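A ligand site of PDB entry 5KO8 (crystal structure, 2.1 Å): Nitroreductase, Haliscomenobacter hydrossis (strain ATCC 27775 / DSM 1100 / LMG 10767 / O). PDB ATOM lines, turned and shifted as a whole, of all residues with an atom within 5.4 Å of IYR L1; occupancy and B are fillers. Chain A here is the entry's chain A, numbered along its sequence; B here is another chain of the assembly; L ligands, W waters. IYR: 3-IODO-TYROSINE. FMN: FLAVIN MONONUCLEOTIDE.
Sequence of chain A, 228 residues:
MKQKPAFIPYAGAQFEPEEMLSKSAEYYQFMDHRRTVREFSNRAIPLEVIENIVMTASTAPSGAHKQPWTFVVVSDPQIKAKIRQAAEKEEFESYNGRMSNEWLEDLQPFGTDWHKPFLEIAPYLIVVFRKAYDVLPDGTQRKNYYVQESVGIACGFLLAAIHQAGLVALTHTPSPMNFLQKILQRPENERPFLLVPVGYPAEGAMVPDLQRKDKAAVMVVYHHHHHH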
ATOM      1  N   ARG A  38      -7.763   4.198 -14.924  1.00  0.00           N
ATOM      2  CA  ARG A  38      -7.376   5.541 -14.509  1.00  0.00           C
ATOM      3  C   ARG A  38      -7.254   6.514 -15.688  1.00  0.00           C
ATOM      4  O   ARG A  38      -7.048   7.707 -15.482  1.00  0.00           O
ATOM      5  CB  ARG A  38      -6.066   5.488 -13.723  1.00  0.00           C
ATOM      6  CG  ARG A  38      -6.176   4.622 -12.469  1.00  0.00           C
ATOM      7  CD  ARG A  38      -4.938   4.675 -11.597  1.00  0.00           C
ATOM      8  NE  ARG A  38      -5.145   3.972 -10.331  1.00  0.00           N
ATOM      9  CZ  ARG A  38      -5.056   2.656 -10.178  1.00  0.00           C
ATOM     10  NH1 ARG A  38      -4.773   1.872 -11.207  1.00  0.00           N
ATOM     11  NH2 ARG A  38      -5.260   2.112  -8.977  1.00  0.00           N
ATOM     12  N   GLU A  91      -2.668  15.422  -2.350  1.00  0.00           N
ATOM     13  CA  GLU A  91      -1.808  14.304  -2.720  1.00  0.00           C
ATOM     14  C   GLU A  91      -0.366  14.721  -2.871  1.00  0.00           C
ATOM     15  O   GLU A  91       0.540  13.946  -2.594  1.00  0.00           O
ATOM     16  CB  GLU A  91      -2.293  13.684  -4.022  1.00  0.00           C
ATOM     17  CG  GLU A  91      -3.665  13.116  -3.912  1.00  0.00           C
ATOM     18  CD  GLU A  91      -3.683  11.701  -3.385  1.00  0.00           C
ATOM     19  OE1 GLU A  91      -2.753  11.334  -2.624  1.00  0.00           O
ATOM     20  OE2 GLU A  91      -4.625  10.958  -3.729  1.00  0.00           O
ATOM     21  N   TYR A  95       2.507  12.621  -1.088  1.00  0.00           N
ATOM     22  CA  TYR A  95       3.540  11.897  -1.821  1.00  0.00           C
ATOM     23  C   TYR A  95       4.966  12.316  -1.423  1.00  0.00           C
ATOM     24  O   TYR A  95       5.941  11.787  -1.963  1.00  0.00           O
ATOM     25  CB  TYR A  95       3.351  12.090  -3.332  1.00  0.00           C
ATOM     26  CG  TYR A  95       2.598  10.950  -3.983  1.00  0.00           C
ATOM     27  CD1 TYR A  95       3.249   9.797  -4.403  1.00  0.00           C
ATOM     28  CD2 TYR A  95       1.226  11.026  -4.174  1.00  0.00           C
ATOM     29  CE1 TYR A  95       2.565   8.756  -4.999  1.00  0.00           C
ATOM     30  CE2 TYR A  95       0.524   9.991  -4.766  1.00  0.00           C
ATOM     31  CZ  TYR A  95       1.194   8.860  -5.180  1.00  0.00           C
ATOM     32  OH  TYR A  95       0.506   7.835  -5.770  1.00  0.00           O
ATOM     33  N   TRP A 103       3.841   2.841   2.781  1.00  0.00           N
ATOM     34  CA  TRP A 103       2.847   3.179   1.777  1.00  0.00           C
ATOM     35  C   TRP A 103       3.438   3.244   0.376  1.00  0.00           C
ATOM     36  O   TRP A 103       2.941   2.612  -0.549  1.00  0.00           O
ATOM     37  CB  TRP A 103       2.207   4.522   2.126  1.00  0.00           C
ATOM     38  CG  TRP A 103       0.809   4.715   1.655  1.00  0.00           C
ATOM     39  CD1 TRP A 103      -0.132   3.741   1.478  1.00  0.00           C
ATOM     40  CD2 TRP A 103       0.189   5.956   1.312  1.00  0.00           C
ATOM     41  NE1 TRP A 103      -1.309   4.317   1.041  1.00  0.00           N
ATOM     42  CE2 TRP A 103      -1.137   5.666   0.929  1.00  0.00           C
ATOM     43  CE3 TRP A 103       0.628   7.290   1.283  1.00  0.00           C
ATOM     44  CZ2 TRP A 103      -2.026   6.659   0.531  1.00  0.00           C
ATOM     45  CZ3 TRP A 103      -0.253   8.272   0.887  1.00  0.00           C
ATOM     46  CH2 TRP A 103      -1.575   7.953   0.517  1.00  0.00           C
ATOM     47  N   LEU A 107       2.574   1.221  -3.146  1.00  0.00           N
ATOM     48  CA  LEU A 107       1.962   1.930  -4.272  1.00  0.00           C
ATOM     49  C   LEU A 107       2.750   1.825  -5.581  1.00  0.00           C
ATOM     50  O   LEU A 107       2.257   2.214  -6.642  1.00  0.00           O
ATOM     51  CB  LEU A 107       1.780   3.411  -3.919  1.00  0.00           C
ATOM     52  CG  LEU A 107       0.820   3.723  -2.776  1.00  0.00           C
ATOM     53  CD1 LEU A 107       0.786   5.224  -2.506  1.00  0.00           C
ATOM     54  CD2 LEU A 107      -0.570   3.208  -3.085  1.00  0.00           C
ATOM     55  N   PHE A 110       1.382   0.573  -9.252  1.00  0.00           N
ATOM     56  CA  PHE A 110       0.245   1.231  -9.885  1.00  0.00           C
ATOM     57  C   PHE A 110       0.644   2.442 -10.725  1.00  0.00           C
ATOM     58  O   PHE A 110      -0.119   2.893 -11.571  1.00  0.00           O
ATOM     59  CB  PHE A 110      -0.766   1.649  -8.817  1.00  0.00           C
ATOM     60  CG  PHE A 110      -1.119   0.551  -7.860  1.00  0.00           C
ATOM     61  CD1 PHE A 110      -1.799  -0.570  -8.303  1.00  0.00           C
ATOM     62  CD2 PHE A 110      -0.748   0.630  -6.529  1.00  0.00           C
ATOM     63  CE1 PHE A 110      -2.114  -1.590  -7.422  1.00  0.00           C
ATOM     64  CE2 PHE A 110      -1.063  -0.390  -5.649  1.00  0.00           C
ATOM     65  CZ  PHE A 110      -1.741  -1.501  -6.096  1.00  0.00           C
ATOM     66  N   THR A 112       1.041   5.637 -10.058  1.00  0.00           N
ATOM     67  CA  THR A 112       0.247   6.848  -9.877  1.00  0.00           C
ATOM     68  C   THR A 112       1.086   7.985  -9.308  1.00  0.00           C
ATOM     69  O   THR A 112       1.909   7.780  -8.412  1.00  0.00           O
ATOM     70  CB  THR A 112      -0.942   6.593  -8.940  1.00  0.00           C
ATOM     71  OG1 THR A 112      -0.500   5.893  -7.770  1.00  0.00           O
ATOM     72  CG2 THR A 112      -2.005   5.779  -9.648  1.00  0.00           C
ATOM     73  N   ASP A 113       0.876   9.181  -9.849  1.00  0.00           N
ATOM     74  CA  ASP A 113       1.459  10.414  -9.336  1.00  0.00           C
ATOM     75  C   ASP A 113       0.418  11.127  -8.500  1.00  0.00           C
ATOM     76  O   ASP A 113      -0.640  10.576  -8.212  1.00  0.00           O
ATOM     77  CB  ASP A 113       1.929  11.322 -10.477  1.00  0.00           C
ATOM     78  CG  ASP A 113       2.887  10.645 -11.425  1.00  0.00           C
ATOM     79  OD1 ASP A 113       3.622   9.739 -10.980  1.00  0.00           O
ATOM     80  OD2 ASP A 113       2.922  11.021 -12.608  1.00  0.00           O
ATOM     81  N   LYS A 116      -4.140  14.039 -11.407  1.00  0.00           N
ATOM     82  CA  LYS A 116      -5.483  13.453 -11.491  1.00  0.00           C
ATOM     83  C   LYS A 116      -6.341  14.077 -12.580  1.00  0.00           C
ATOM     84  O   LYS A 116      -7.393  14.642 -12.295  1.00  0.00           O
ATOM     85  CB  LYS A 116      -6.192  13.614 -10.158  1.00  0.00           C
ATOM     86  CG  LYS A 116      -5.454  12.968  -9.044  1.00  0.00           C
ATOM     87  CD  LYS A 116      -6.302  12.863  -7.824  1.00  0.00           C
ATOM     88  CE  LYS A 116      -5.447  12.453  -6.681  1.00  0.00           C
ATOM     89  NZ  LYS A 116      -4.681  11.192  -6.944  1.00  0.00           N
ATOM     90  N   HIS A 172     -11.846   5.926  -5.750  1.00  0.00           N
ATOM     91  CA  HIS A 172     -10.852   6.867  -5.213  1.00  0.00           C
ATOM     92  C   HIS A 172     -11.195   7.312  -3.789  1.00  0.00           C
ATOM     93  O   HIS A 172     -12.367   7.453  -3.434  1.00  0.00           O
ATOM     94  CB  HIS A 172     -10.747   8.083  -6.144  1.00  0.00           C
ATOM     95  CG  HIS A 172      -9.423   8.791  -6.075  1.00  0.00           C
ATOM     96  ND1 HIS A 172      -9.142   9.718  -5.102  1.00  0.00           N
ATOM     97  CD2 HIS A 172      -8.324   8.701  -6.848  1.00  0.00           C
ATOM     98  CE1 HIS A 172      -7.910  10.181  -5.281  1.00  0.00           C
ATOM     99  NE2 HIS A 172      -7.392   9.571  -6.336  1.00  0.00           N
ATOM    100  N   THR A 173     -10.158   7.529  -2.980  1.00  0.00           N
ATOM    101  CA  THR A 173     -10.351   8.017  -1.615  1.00  0.00           C
ATOM    102  C   THR A 173     -11.054   9.369  -1.633  1.00  0.00           C
ATOM    103  O   THR A 173     -10.844  10.167  -2.554  1.00  0.00           O
ATOM    104  CB  THR A 173      -9.027   8.156  -0.854  1.00  0.00           C
ATOM    105  OG1 THR A 173      -8.163   9.069  -1.537  1.00  0.00           O
ATOM    106  CG2 THR A 173      -8.348   6.804  -0.720  1.00  0.00           C
ATOM    107  N   SER A 175     -10.568  12.238  -0.603  1.00  0.00           N
ATOM    108  CA  SER A 175      -9.684  13.342  -0.227  1.00  0.00           C
ATOM    109  C   SER A 175      -9.725  14.432  -1.309  1.00  0.00           C
ATOM    110  O   SER A 175      -9.714  14.108  -2.497  1.00  0.00           O
ATOM    111  CB  SER A 175      -8.256  12.840  -0.037  1.00  0.00           C
ATOM    112  OG  SER A 175      -7.862  11.979  -1.087  1.00  0.00           O
ATOM    113  N   SER B  62      -9.739  -2.950  -4.116  1.00  0.00           N
ATOM    114  CA  SER B  62      -9.308  -2.822  -2.739  1.00  0.00           C
ATOM    115  C   SER B  62      -8.118  -1.881  -2.604  1.00  0.00           C
ATOM    116  O   SER B  62      -7.297  -1.763  -3.535  1.00  0.00           O
ATOM    117  CB  SER B  62      -8.949  -4.194  -2.154  1.00  0.00           C
ATOM    118  OG  SER B  62      -7.815  -4.735  -2.814  1.00  0.00           O
ATOM    119  N   GLY B  63      -8.016  -1.209  -1.461  1.00  0.00           N
ATOM    120  CA  GLY B  63      -6.914  -0.296  -1.216  1.00  0.00           C
ATOM    121  C   GLY B  63      -5.572  -0.945  -1.453  1.00  0.00           C
ATOM    122  O   GLY B  63      -5.239  -1.954  -0.802  1.00  0.00           O
ATOM    123  N   ALA B  64      -4.813  -0.401  -2.404  1.00  0.00           N
ATOM    124  CA  ALA B  64      -3.468  -0.876  -2.723  1.00  0.00           C
ATOM    125  C   ALA B  64      -3.455  -2.345  -3.152  1.00  0.00           C
ATOM    126  O   ALA B  64      -2.435  -3.027  -3.049  1.00  0.00           O
ATOM    127  CB  ALA B  64      -2.526  -0.682  -1.544  1.00  0.00           C
ATOM    128  N   HIS B  65      -4.606  -2.821  -3.627  1.00  0.00           N
ATOM    129  CA  HIS B  65      -4.743  -4.210  -4.066  1.00  0.00           C
ATOM    130  C   HIS B  65      -4.359  -5.200  -2.961  1.00  0.00           C
ATOM    131  O   HIS B  65      -3.741  -6.223  -3.216  1.00  0.00           O
ATOM    132  CB  HIS B  65      -3.878  -4.459  -5.317  1.00  0.00           C
ATOM    133  CG  HIS B  65      -4.104  -5.791  -5.957  1.00  0.00           C
ATOM    134  ND1 HIS B  65      -5.372  -6.317  -6.159  1.00  0.00           N
ATOM    135  CD2 HIS B  65      -3.239  -6.732  -6.401  1.00  0.00           C
ATOM    136  CE1 HIS B  65      -5.268  -7.510  -6.708  1.00  0.00           C
ATOM    137  NE2 HIS B  65      -3.980  -7.786  -6.872  1.00  0.00           N
ATOM    138  N   TYR B 145      -5.047  -0.615   3.888  1.00  0.00           N
ATOM    139  CA  TYR B 145      -5.637   0.715   3.869  1.00  0.00           C
ATOM    140  C   TYR B 145      -7.074   0.702   3.344  1.00  0.00           C
ATOM    141  O   TYR B 145      -7.398  -0.017   2.400  1.00  0.00           O
ATOM    142  CB  TYR B 145      -4.768   1.642   3.023  1.00  0.00           C
ATOM    143  CG  TYR B 145      -3.310   1.587   3.429  1.00  0.00           C
ATOM    144  CD1 TYR B 145      -2.856   2.310   4.530  1.00  0.00           C
ATOM    145  CD2 TYR B 145      -2.396   0.807   2.725  1.00  0.00           C
ATOM    146  CE1 TYR B 145      -1.522   2.255   4.917  1.00  0.00           C
ATOM    147  CE2 TYR B 145      -1.065   0.757   3.098  1.00  0.00           C
ATOM    148  CZ  TYR B 145      -0.632   1.483   4.196  1.00  0.00           C
ATOM    149  OH  TYR B 145       0.689   1.427   4.576  1.00  0.00           O
ATOM    150  N   TYR B 146      -7.906   1.514   3.988  1.00  0.00           N
ATOM    151  CA  TYR B 146      -9.322   1.631   3.666  1.00  0.00           C
ATOM    152  C   TYR B 146      -9.959   0.248   3.623  1.00  0.00           C
ATOM    153  O   TYR B 146     -10.605  -0.133   2.643  1.00  0.00           O
ATOM    154  CB  TYR B 146      -9.512   2.391   2.351  1.00  0.00           C
ATOM    155  CG  TYR B 146      -9.037   3.826   2.414  1.00  0.00           C
ATOM    156  CD1 TYR B 146      -9.874   4.833   2.885  1.00  0.00           C
ATOM    157  CD2 TYR B 146      -7.754   4.179   2.029  1.00  0.00           C
ATOM    158  CE1 TYR B 146      -9.445   6.147   2.965  1.00  0.00           C
ATOM    159  CE2 TYR B 146      -7.315   5.499   2.101  1.00  0.00           C
ATOM    160  CZ  TYR B 146      -8.172   6.475   2.572  1.00  0.00           C
ATOM    161  OH  TYR B 146      -7.747   7.785   2.643  1.00  0.00           O
HETATM  162  N   IYR L   1      -4.861   8.334  -3.313  1.00  0.00           N
HETATM  163  CA  IYR L   1      -3.508   8.247  -3.828  1.00  0.00           C
HETATM  164  CB  IYR L   1      -2.654   7.062  -3.326  1.00  0.00           C
HETATM  165  CC  IYR L   1      -3.298   5.727  -3.495  1.00  0.00           C
HETATM  166  CD  IYR L   1      -4.008   5.149  -2.442  1.00  0.00           C
HETATM  167  CE  IYR L   1      -4.620   3.886  -2.575  1.00  0.00           C
HETATM  168  IE  IYR L   1      -5.623   3.161  -0.977  1.00  0.00           I
HETATM  169  CF  IYR L   1      -4.506   3.203  -3.792  1.00  0.00           C
HETATM  170  OF  IYR L   1      -5.056   1.971  -4.060  1.00  0.00           O
HETATM  171  CG  IYR L   1      -3.788   3.783  -4.861  1.00  0.00           C
HETATM  172  CH  IYR L   1      -3.190   5.024  -4.711  1.00  0.00           C
HETATM  173  C   IYR L   1      -3.570   8.272  -5.350  1.00  0.00           C
HETATM  174  O   IYR L   1      -4.569   8.362  -6.070  1.00  0.00           O
HETATM  175  OXT IYR L   1      -2.360   8.206  -5.980  1.00  0.00           O
HETATM  176  N1  FMN L   2      -6.687   3.882  -6.855  1.00  0.00           N
HETATM  177  C2  FMN L   2      -5.959   5.053  -7.023  1.00  0.00           C
HETATM  178  O2  FMN L   2      -5.268   5.199  -8.030  1.00  0.00           O
HETATM  179  N3  FMN L   2      -5.999   6.034  -6.059  1.00  0.00           N
HETATM  180  C4  FMN L   2      -6.774   5.864  -4.934  1.00  0.00           C
HETATM  181  O4  FMN L   2      -6.809   6.758  -4.085  1.00  0.00           O
HETATM  182  C4A FMN L   2      -7.512   4.696  -4.763  1.00  0.00           C
HETATM  183  N5  FMN L   2      -8.285   4.522  -3.625  1.00  0.00           N
HETATM  184  C5A FMN L   2      -9.017   3.366  -3.450  1.00  0.00           C
HETATM  185  C6  FMN L   2      -9.802   3.219  -2.308  1.00  0.00           C
HETATM  186  C7  FMN L   2     -10.551   2.065  -2.115  1.00  0.00           C
HETATM  187  C7M FMN L   2     -11.380   1.927  -0.864  1.00  0.00           C
HETATM  188  C8  FMN L   2     -10.508   1.060  -3.081  1.00  0.00           C
HETATM  189  C8M FMN L   2     -11.307  -0.192  -2.916  1.00  0.00           C
HETATM  190  C9  FMN L   2      -9.731   1.219  -4.225  1.00  0.00           C
HETATM  191  C9A FMN L   2      -8.973   2.370  -4.420  1.00  0.00           C
HETATM  192  N10 FMN L   2      -8.196   2.529  -5.565  1.00  0.00           N
HETATM  193  C10 FMN L   2      -7.467   3.700  -5.733  1.00  0.00           C
HETATM  194  C1' FMN L   2      -8.142   1.469  -6.628  1.00  0.00           C
HETATM  195  C2' FMN L   2      -7.259   0.285  -6.221  1.00  0.00           C
HETATM  196  O2' FMN L   2      -5.896   0.677  -6.232  1.00  0.00           O
HETATM  197  C3' FMN L   2      -7.493  -0.903  -7.149  1.00  0.00           C
HETATM  198  O3' FMN L   2      -8.812  -1.337  -6.924  1.00  0.00           O
HETATM  199  C4' FMN L   2      -6.491  -2.030  -6.937  1.00  0.00           C
HETATM  200  O4' FMN L   2      -5.209  -1.608  -7.366  1.00  0.00           O
HETATM  201  C5' FMN L   2      -6.867  -3.315  -7.667  1.00  0.00           C
HETATM  202  O5' FMN L   2      -7.097  -3.089  -9.046  1.00  0.00           O
HETATM  203  P   FMN L   2      -8.454  -3.649  -9.702  1.00  0.00           P
HETATM  204  O1P FMN L   2      -8.393  -3.375 -11.191  1.00  0.00           O
HETATM  205  O2P FMN L   2      -9.612  -2.910  -9.089  1.00  0.00           O
HETATM  206  O3P FMN L   2      -8.604  -5.125  -9.434  1.00  0.00           O
HETATM  207  O   HOH W   1      -4.507   8.200  -0.198  1.00  0.00           O
HETATM  208  O   HOH W   2      -4.869   7.754  -9.132  1.00  0.00           O
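O4 of FMN L2 is in hydrogen-bond range of N of IYR L1 (2.6 Å).
Residues that only touch IYR L1: Leu 107 (3.6 Å), Asp 113 (3.7 Å), Gly 63 of chain B (3.7 Å), Thr 173 (3.8 Å), Tyr 146 of chain B (3.8 Å) and Trp 103 (3.9 Å).
Hydrophobic or aromatic side chains that line IYR L1: Tyr 95, Trp 103, Leu 107, His 172 and Tyr 146 of chain B.
Within 4 Å of IYR L1: Glu 91, Tyr 95, Trp 103, Leu 107, Thr 112, Asp 113, Lys 116, His 172, Thr 173, Gly 63 of chain B, Ala 64 of chain B and Tyr 146 of chain B.
The nearest printed residue that does not touch IYR L1 is Tyr 145 of chain B (4.4 Å).
Water W2 bridges O2 of FMN L2 (2.8 Å) and O of IYR L1 (3.1 Å).
An oxygen (O) of IYR L1 is in salt-bridge range of the side-chain amino group of Lys 116, at 3.0 Å.
N of Ala 64 of chain B sits at hydrogen-bond distance from OF of IYR L1 (2.9 Å).
The side-chain carboxylate of Glu 91 is in salt-bridge range of a nitrogen (N) of IYR L1 (2.7 Å).
A ring nitrogen (NE2) of His 172 sits at hydrogen-bond distance from an oxygen (O) of IYR L1 (3.1 Å).
The side-chain hydroxyl (OG1) of Thr 112 sits at hydrogen-bond distance from an oxygen (OXT) of IYR L1 (3.5 Å).
An oxygen (O3') of FMN L2 is in hydrogen-bond range of the backbone NH of Ser 62 of chain B, at 3.4 Å.
O2 of FMN L2 sits at hydrogen-bond distance from NE of Arg 38, at 2.6 Å.
The side-chain hydroxyl of Tyr 95 lies within hydrogen-bond range of an oxygen (OXT) of IYR L1 (2.9 Å).
NE2 of His 172 lies within hydrogen-bond range of NZ of Lys 116 (3.2 Å).
The side-chain hydroxyl (OG1) of Thr 173 is in hydrogen-bond range of the side-chain hydroxyl (OG) of Ser 175 (3.0 Å).
The side-chain carboxylate (OE2) of Glu 91 lies within salt-bridge range of the side-chain amino group (NZ) of Lys 116 (3.2 Å).
The side-chain hydroxyl (OH) of Tyr 95 is in hydrogen-bond range of the side-chain hydroxyl (OG1) of Thr 112, 3.0 Å away.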
